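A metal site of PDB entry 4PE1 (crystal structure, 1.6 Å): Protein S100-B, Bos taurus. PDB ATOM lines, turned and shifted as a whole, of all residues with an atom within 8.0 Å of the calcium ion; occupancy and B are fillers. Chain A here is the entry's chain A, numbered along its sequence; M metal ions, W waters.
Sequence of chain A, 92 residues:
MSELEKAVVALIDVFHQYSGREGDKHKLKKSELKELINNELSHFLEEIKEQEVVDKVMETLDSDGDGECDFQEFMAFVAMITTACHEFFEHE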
ATOM      1  N   PHE A  15     -29.584 -21.764  -5.516  1.00  0.00           N
ATOM      2  CA  PHE A  15     -29.087 -23.066  -5.973  1.00  0.00           C
ATOM      3  C   PHE A  15     -30.215 -23.945  -6.525  1.00  0.00           C
ATOM      4  O   PHE A  15     -30.053 -24.559  -7.584  1.00  0.00           O
ATOM      5  CB  PHE A  15     -28.347 -23.830  -4.865  1.00  0.00           C
ATOM      6  CG  PHE A  15     -27.786 -25.138  -5.333  1.00  0.00           C
ATOM      7  CD1 PHE A  15     -26.526 -25.203  -5.926  1.00  0.00           C
ATOM      8  CD2 PHE A  15     -28.531 -26.314  -5.244  1.00  0.00           C
ATOM      9  CE1 PHE A  15     -26.004 -26.405  -6.384  1.00  0.00           C
ATOM     10  CE2 PHE A  15     -28.016 -27.525  -5.711  1.00  0.00           C
ATOM     11  CZ  PHE A  15     -26.755 -27.572  -6.266  1.00  0.00           C
ATOM     12  N   HIS A  16     -31.324 -24.003  -5.804  1.00  0.00           N
ATOM     13  CA  HIS A  16     -32.468 -24.816  -6.191  1.00  0.00           C
ATOM     14  C   HIS A  16     -33.004 -24.347  -7.538  1.00  0.00           C
ATOM     15  O   HIS A  16     -33.331 -25.165  -8.407  1.00  0.00           O
ATOM     16  CB  HIS A  16     -33.568 -24.724  -5.124  1.00  0.00           C
ATOM     17  CG  HIS A  16     -34.865 -25.378  -5.501  1.00  0.00           C
ATOM     18  ND1 HIS A  16     -35.112 -26.717  -5.293  1.00  0.00           N
ATOM     19  CD2 HIS A  16     -35.980 -24.864  -6.067  1.00  0.00           C
ATOM     20  CE1 HIS A  16     -36.331 -27.010  -5.721  1.00  0.00           C
ATOM     21  NE2 HIS A  16     -36.873 -25.905  -6.198  1.00  0.00           N
ATOM     22  N   GLN A  17     -33.081 -23.031  -7.721  1.00  0.00           N
ATOM     23  CA  GLN A  17     -33.608 -22.487  -8.966  1.00  0.00           C
ATOM     24  C   GLN A  17     -32.773 -22.873 -10.174  1.00  0.00           C
ATOM     25  O   GLN A  17     -33.292 -23.377 -11.169  1.00  0.00           O
ATOM     26  CB  GLN A  17     -33.717 -20.969  -8.898  1.00  0.00           C
ATOM     27  CG  GLN A  17     -34.822 -20.467  -7.984  1.00  0.00           C
ATOM     28  CD  GLN A  17     -34.739 -18.968  -7.749  1.00  0.00           C
ATOM     29  OE1 GLN A  17     -33.809 -18.307  -8.224  1.00  0.00           O
ATOM     30  NE2 GLN A  17     -35.704 -18.429  -7.015  1.00  0.00           N
ATOM     31  N   TYR A  18     -31.473 -22.645 -10.074  1.00  0.00           N
ATOM     32  CA  TYR A  18     -30.582 -22.905 -11.186  1.00  0.00           C
ATOM     33  C   TYR A  18     -30.319 -24.385 -11.425  1.00  0.00           C
ATOM     34  O   TYR A  18     -30.294 -24.830 -12.577  1.00  0.00           O
ATOM     35  CB  TYR A  18     -29.278 -22.084 -11.047  1.00  0.00           C
ATOM     36  CG  TYR A  18     -29.483 -20.658 -11.499  1.00  0.00           C
ATOM     37  CD1 TYR A  18     -29.960 -19.689 -10.627  1.00  0.00           C
ATOM     38  CD2 TYR A  18     -29.243 -20.294 -12.824  1.00  0.00           C
ATOM     39  CE1 TYR A  18     -30.174 -18.389 -11.055  1.00  0.00           C
ATOM     40  CE2 TYR A  18     -29.450 -18.987 -13.253  1.00  0.00           C
ATOM     41  CZ  TYR A  18     -29.911 -18.044 -12.358  1.00  0.00           C
ATOM     42  OH  TYR A  18     -30.138 -16.758 -12.775  1.00  0.00           O
ATOM     43  N   SER A  19     -30.166 -25.167 -10.354  1.00  0.00           N
ATOM     44  CA  SER A  19     -29.871 -26.591 -10.478  1.00  0.00           C
ATOM     45  C   SER A  19     -31.075 -27.319 -11.053  1.00  0.00           C
ATOM     46  O   SER A  19     -30.921 -28.343 -11.727  1.00  0.00           O
ATOM     47  CB  SER A  19     -29.486 -27.207  -9.121  1.00  0.00           C
ATOM     48  OG  SER A  19     -30.597 -27.257  -8.250  1.00  0.00           O
ATOM     49  N   GLY A  20     -32.271 -26.796 -10.812  1.00  0.00           N
ATOM     50  CA  GLY A  20     -33.490 -27.498 -11.198  1.00  0.00           C
ATOM     51  C   GLY A  20     -33.908 -27.290 -12.642  1.00  0.00           C
ATOM     52  O   GLY A  20     -34.914 -27.857 -13.100  1.00  0.00           O
ATOM     53  N   ARG A  21     -33.142 -26.486 -13.387  1.00  0.00           N
ATOM     54  CA  ARG A  21     -33.518 -26.171 -14.764  1.00  0.00           C
ATOM     55  C   ARG A  21     -33.452 -27.391 -15.667  1.00  0.00           C
ATOM     56  O   ARG A  21     -34.395 -27.660 -16.439  1.00  0.00           O
ATOM     57  CB  ARG A  21     -32.619 -25.064 -15.314  1.00  0.00           C
ATOM     58  CG  ARG A  21     -32.900 -23.698 -14.721  1.00  0.00           C
ATOM     59  CD  ARG A  21     -31.906 -22.679 -15.256  1.00  0.00           C
ATOM     60  NE  ARG A  21     -32.276 -21.306 -14.921  1.00  0.00           N
ATOM     61  CZ  ARG A  21     -31.745 -20.230 -15.505  1.00  0.00           C
ATOM     62  NH1 ARG A  21     -30.843 -20.380 -16.448  1.00  0.00           N
ATOM     63  NH2 ARG A  21     -32.137 -19.014 -15.154  1.00  0.00           N
ATOM     64  N   GLU A  22     -32.350 -28.113 -15.592  1.00  0.00           N
ATOM     65  CA  GLU A  22     -32.096 -29.234 -16.491  1.00  0.00           C
ATOM     66  C   GLU A  22     -31.416 -30.430 -15.829  1.00  0.00           C
ATOM     67  O   GLU A  22     -30.728 -30.300 -14.801  1.00  0.00           O
ATOM     68  CB  GLU A  22     -31.230 -28.762 -17.668  1.00  0.00           C
ATOM     69  CG  GLU A  22     -31.921 -27.818 -18.626  1.00  0.00           C
ATOM     70  CD  GLU A  22     -31.046 -27.422 -19.796  1.00  0.00           C
ATOM     71  OE1 GLU A  22     -30.238 -28.258 -20.252  1.00  0.00           O
ATOM     72  OE2 GLU A  22     -31.157 -26.263 -20.244  1.00  0.00           O
ATOM     73  N   GLY A  23     -31.602 -31.595 -16.446  1.00  0.00           N
ATOM     74  CA  GLY A  23     -30.911 -32.809 -16.044  1.00  0.00           C
ATOM     75  C   GLY A  23     -31.075 -33.141 -14.575  1.00  0.00           C
ATOM     76  O   GLY A  23     -32.202 -33.143 -14.060  1.00  0.00           O
ATOM     77  N   ASP A  24     -29.956 -33.440 -13.921  1.00  0.00           N
ATOM     78  CA  ASP A  24     -29.934 -33.662 -12.480  1.00  0.00           C
ATOM     79  C   ASP A  24     -30.457 -32.403 -11.817  1.00  0.00           C
ATOM     80  O   ASP A  24     -29.874 -31.317 -11.971  1.00  0.00           O
ATOM     81  CB  ASP A  24     -28.512 -33.954 -12.009  1.00  0.00           C
ATOM     82  CG  ASP A  24     -28.453 -34.461 -10.591  1.00  0.00           C
ATOM     83  OD1 ASP A  24     -29.330 -34.102  -9.761  1.00  0.00           O
ATOM     84  OD2 ASP A  24     -27.531 -35.245 -10.292  1.00  0.00           O
ATOM     85  N   LYS A  25     -31.557 -32.540 -11.098  1.00  0.00           N
ATOM     86  CA  LYS A  25     -32.264 -31.397 -10.527  1.00  0.00           C
ATOM     87  C   LYS A  25     -31.619 -30.901  -9.244  1.00  0.00           C
ATOM     88  O   LYS A  25     -32.047 -29.886  -8.689  1.00  0.00           O
ATOM     89  CB  LYS A  25     -33.721 -31.783 -10.252  1.00  0.00           C
ATOM     90  CG  LYS A  25     -34.473 -32.188 -11.511  1.00  0.00           C
ATOM     91  CD  LYS A  25     -35.132 -30.985 -12.175  1.00  0.00           C
ATOM     92  CE  LYS A  25     -36.206 -30.376 -11.273  1.00  0.00           C
ATOM     93  NZ  LYS A  25     -36.841 -29.156 -11.849  1.00  0.00           N
ATOM     94  N   HIS A  26     -30.594 -31.607  -8.776  1.00  0.00           N
ATOM     95  CA  HIS A  26     -29.934 -31.215  -7.543  1.00  0.00           C
ATOM     96  C   HIS A  26     -28.492 -30.828  -7.807  1.00  0.00           C
ATOM     97  O   HIS A  26     -27.702 -30.655  -6.878  1.00  0.00           O
ATOM     98  CB  HIS A  26     -29.993 -32.343  -6.518  1.00  0.00           C
ATOM     99  CG  HIS A  26     -31.389 -32.763  -6.172  1.00  0.00           C
ATOM    100  ND1 HIS A  26     -31.710 -34.055  -5.835  1.00  0.00           N
ATOM    101  CD2 HIS A  26     -32.541 -32.058  -6.112  1.00  0.00           C
ATOM    102  CE1 HIS A  26     -33.000 -34.132  -5.579  1.00  0.00           C
ATOM    103  NE2 HIS A  26     -33.526 -32.930  -5.744  1.00  0.00           N
ATOM    104  N   LYS A  27     -28.129 -30.697  -9.081  1.00  0.00           N
ATOM    105  CA  LYS A  27     -26.784 -30.246  -9.449  1.00  0.00           C
ATOM    106  C   LYS A  27     -26.805 -29.193 -10.553  1.00  0.00           C
ATOM    107  O   LYS A  27     -27.752 -29.100 -11.333  1.00  0.00           O
ATOM    108  CB  LYS A  27     -25.900 -31.422  -9.852  1.00  0.00           C
ATOM    109  CG  LYS A  27     -25.724 -32.486  -8.773  1.00  0.00           C
ATOM    110  CD  LYS A  27     -24.915 -33.648  -9.286  1.00  0.00           C
ATOM    111  CE  LYS A  27     -24.953 -34.816  -8.318  1.00  0.00           C
ATOM    112  NZ  LYS A  27     -26.358 -35.172  -7.968  1.00  0.00           N
ATOM    113  N   LEU A  28     -25.756 -28.362 -10.587  1.00  0.00           N
ATOM    114  CA  LEU A  28     -25.589 -27.384 -11.650  1.00  0.00           C
ATOM    115  C   LEU A  28     -24.745 -27.960 -12.778  1.00  0.00           C
ATOM    116  O   LEU A  28     -23.572 -28.288 -12.566  1.00  0.00           O
ATOM    117  CB  LEU A  28     -24.906 -26.131 -11.111  1.00  0.00           C
ATOM    118  CG  LEU A  28     -25.612 -25.406  -9.963  1.00  0.00           C
ATOM    119  CD1 LEU A  28     -24.638 -24.418  -9.266  1.00  0.00           C
ATOM    120  CD2 LEU A  28     -26.804 -24.650 -10.500  1.00  0.00           C
ATOM    121  N   LYS A  29     -25.325 -28.117 -13.968  1.00  0.00           N
ATOM    122  CA  LYS A  29     -24.506 -28.428 -15.143  1.00  0.00           C
ATOM    123  C   LYS A  29     -23.806 -27.148 -15.593  1.00  0.00           C
ATOM    124  O   LYS A  29     -24.058 -26.075 -15.031  1.00  0.00           O
ATOM    125  CB  LYS A  29     -25.361 -29.038 -16.286  1.00  0.00           C
ATOM    126  CG  LYS A  29     -26.377 -28.082 -16.881  1.00  0.00           C
ATOM    127  CD  LYS A  29     -27.355 -28.796 -17.817  1.00  0.00           C
ATOM    128  CE  LYS A  29     -26.640 -29.649 -18.831  1.00  0.00           C
ATOM    129  NZ  LYS A  29     -27.595 -30.239 -19.812  1.00  0.00           N
ATOM    130  N   LYS A  30     -22.944 -27.255 -16.589  1.00  0.00           N
ATOM    131  CA  LYS A  30     -22.192 -26.081 -17.060  1.00  0.00           C
ATOM    132  C   LYS A  30     -23.066 -24.901 -17.452  1.00  0.00           C
ATOM    133  O   LYS A  30     -22.776 -23.758 -17.088  1.00  0.00           O
ATOM    134  CB  LYS A  30     -21.272 -26.446 -18.233  1.00  0.00           C
ATOM    135  CG  LYS A  30     -20.082 -27.318 -17.855  1.00  0.00           C
ATOM    136  CD  LYS A  30     -19.334 -27.726 -19.117  1.00  0.00           C
ATOM    137  CE  LYS A  30     -17.998 -28.386 -18.796  1.00  0.00           C
ATOM    138  NZ  LYS A  30     -17.185 -28.562 -20.035  1.00  0.00           N
ATOM    139  N   SER A  31     -24.143 -25.151 -18.202  1.00  0.00           N
ATOM    140  CA  SER A  31     -24.989 -24.061 -18.656  1.00  0.00           C
ATOM    141  C   SER A  31     -25.685 -23.396 -17.482  1.00  0.00           C
ATOM    142  O   SER A  31     -25.858 -22.171 -17.472  1.00  0.00           O
ATOM    143  CB  SER A  31     -26.006 -24.543 -19.685  1.00  0.00           C
ATOM    144  OG  SER A  31     -26.823 -25.547 -19.129  1.00  0.00           O
ATOM    145  N   GLU A  32     -26.066 -24.196 -16.480  1.00  0.00           N
ATOM    146  CA  GLU A  32     -26.728 -23.671 -15.282  1.00  0.00           C
ATOM    147  C   GLU A  32     -25.758 -22.855 -14.457  1.00  0.00           C
ATOM    148  O   GLU A  32     -26.094 -21.762 -14.014  1.00  0.00           O
ATOM    149  CB  GLU A  32     -27.303 -24.821 -14.438  1.00  0.00           C
ATOM    150  CG  GLU A  32     -28.447 -25.567 -15.144  1.00  0.00           C
ATOM    151  CD  GLU A  32     -28.832 -26.844 -14.424  1.00  0.00           C
ATOM    152  OE1 GLU A  32     -27.964 -27.424 -13.722  1.00  0.00           O
ATOM    153  OE2 GLU A  32     -29.998 -27.281 -14.537  1.00  0.00           O
ATOM    154  N   LEU A  33     -24.545 -23.360 -14.258  1.00  0.00           N
ATOM    155  CA  LEU A  33     -23.539 -22.627 -13.485  1.00  0.00           C
ATOM    156  C   LEU A  33     -23.176 -21.312 -14.178  1.00  0.00           C
ATOM    157  O   LEU A  33     -23.062 -20.267 -13.526  1.00  0.00           O
ATOM    158  CB  LEU A  33     -22.299 -23.501 -13.279  1.00  0.00           C
ATOM    159  CG  LEU A  33     -21.106 -22.795 -12.632  1.00  0.00           C
ATOM    160  CD1 LEU A  33     -21.436 -22.411 -11.201  1.00  0.00           C
ATOM    161  CD2 LEU A  33     -19.896 -23.729 -12.660  1.00  0.00           C
ATOM    162  N   GLU A  68     -20.383 -31.765 -12.765  1.00  0.00           N
ATOM    163  CA  GLU A  68     -21.454 -30.888 -12.294  1.00  0.00           C
ATOM    164  C   GLU A  68     -21.093 -30.309 -10.938  1.00  0.00           C
ATOM    165  O   GLU A  68     -20.199 -30.818 -10.244  1.00  0.00           O
ATOM    166  CB  GLU A  68     -22.817 -31.612 -12.229  1.00  0.00           C
ATOM    167  CG  GLU A  68     -23.234 -32.206 -13.581  1.00  0.00           C
ATOM    168  CD  GLU A  68     -24.732 -32.201 -13.848  1.00  0.00           C
ATOM    169  OE1 GLU A  68     -25.487 -31.443 -13.195  1.00  0.00           O
ATOM    170  OE2 GLU A  68     -25.170 -32.950 -14.761  1.00  0.00           O
ATOM    171  N   CYS A  69     -21.770 -29.235 -10.562  1.00  0.00           N
ATOM    172  CA  CYS A  69     -21.553 -28.624  -9.255  1.00  0.00           C
ATOM    173  C   CYS A  69     -22.717 -28.980  -8.361  1.00  0.00           C
ATOM    174  O   CYS A  69     -23.845 -28.533  -8.607  1.00  0.00           O
ATOM    175  CB  CYS A  69     -21.438 -27.102  -9.427  1.00  0.00           C
ATOM    176  SG  CYS A  69     -21.003 -26.187  -7.938  1.00  0.00           S
HETATM  177 CA    CA M   1     -29.375 -29.344 -13.159  1.00  0.00          CA
HETATM  178  O   HOH W   1     -27.724 -30.614 -14.114  1.00  0.00           O
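The side-chain carboxylate (OE1) of Glu 22 is in salt-bridge range of the side-chain amino group (NZ) of Lys 29, 3.3 Å away.
OD1 of Asp 24 is in hydrogen-bond range of N of His 26 (3.0 Å).
The side-chain carboxylate (OD2) of Asp 24 lies within salt-bridge range of the side-chain amino group (NZ) of Lys 27 (2.6 Å).
The side-chain hydroxyl (OG) of Ser 19 is in hydrogen-bond range of the backbone carbonyl oxygen (O) of His 16 (3.4 Å).
N of Lys 29 lies close to OE1 of Glu 32 (2.7 Å).
The backbone carbonyl oxygen (O) of Phe 15 sits at hydrogen-bond distance from the side-chain hydroxyl (OG) of Ser 19, at 2.8 Å.
The backbone carbonyl oxygen (O) of Lys 25 sits at hydrogen-bond distance from the side-chain hydroxyl (OG) of Ser 19, 3.0 Å away.
The side-chain carboxylate (OE2) of Glu 32 lies close to the backbone NH (N) of Arg 21.
Five residues have an atom within 4 Å of the calcium ion: Ser 19, Glu 22, Asp 24, Lys 27 and Glu 32.
The nearest printed residue that does not touch the calcium ion is Lys 29 (4.3 Å).
The calcium ion is bound by water W1, at 2.3 Å.
O of Glu 22 is bound to the calcium ion, at 2.3 Å.
The calcium ion is bound by O of Ser 19 (2.3 Å).
O of Asp 24 is bound to the calcium ion, at 2.4 Å.
OE1 of Glu 32 binds the calcium ion, at 2.4 Å.
O of Lys 27 binds the calcium ion, 2.5 Å away.
OE2 of Glu 32 is bound to the calcium ion.
The calcium ion has seven donor atoms within binding distance.
Water W1 bridges the side-chain carboxylate (OE1) of Glu 68 (2.6 Å) and the backbone NH (N) of Lys 29 (3.5 Å).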
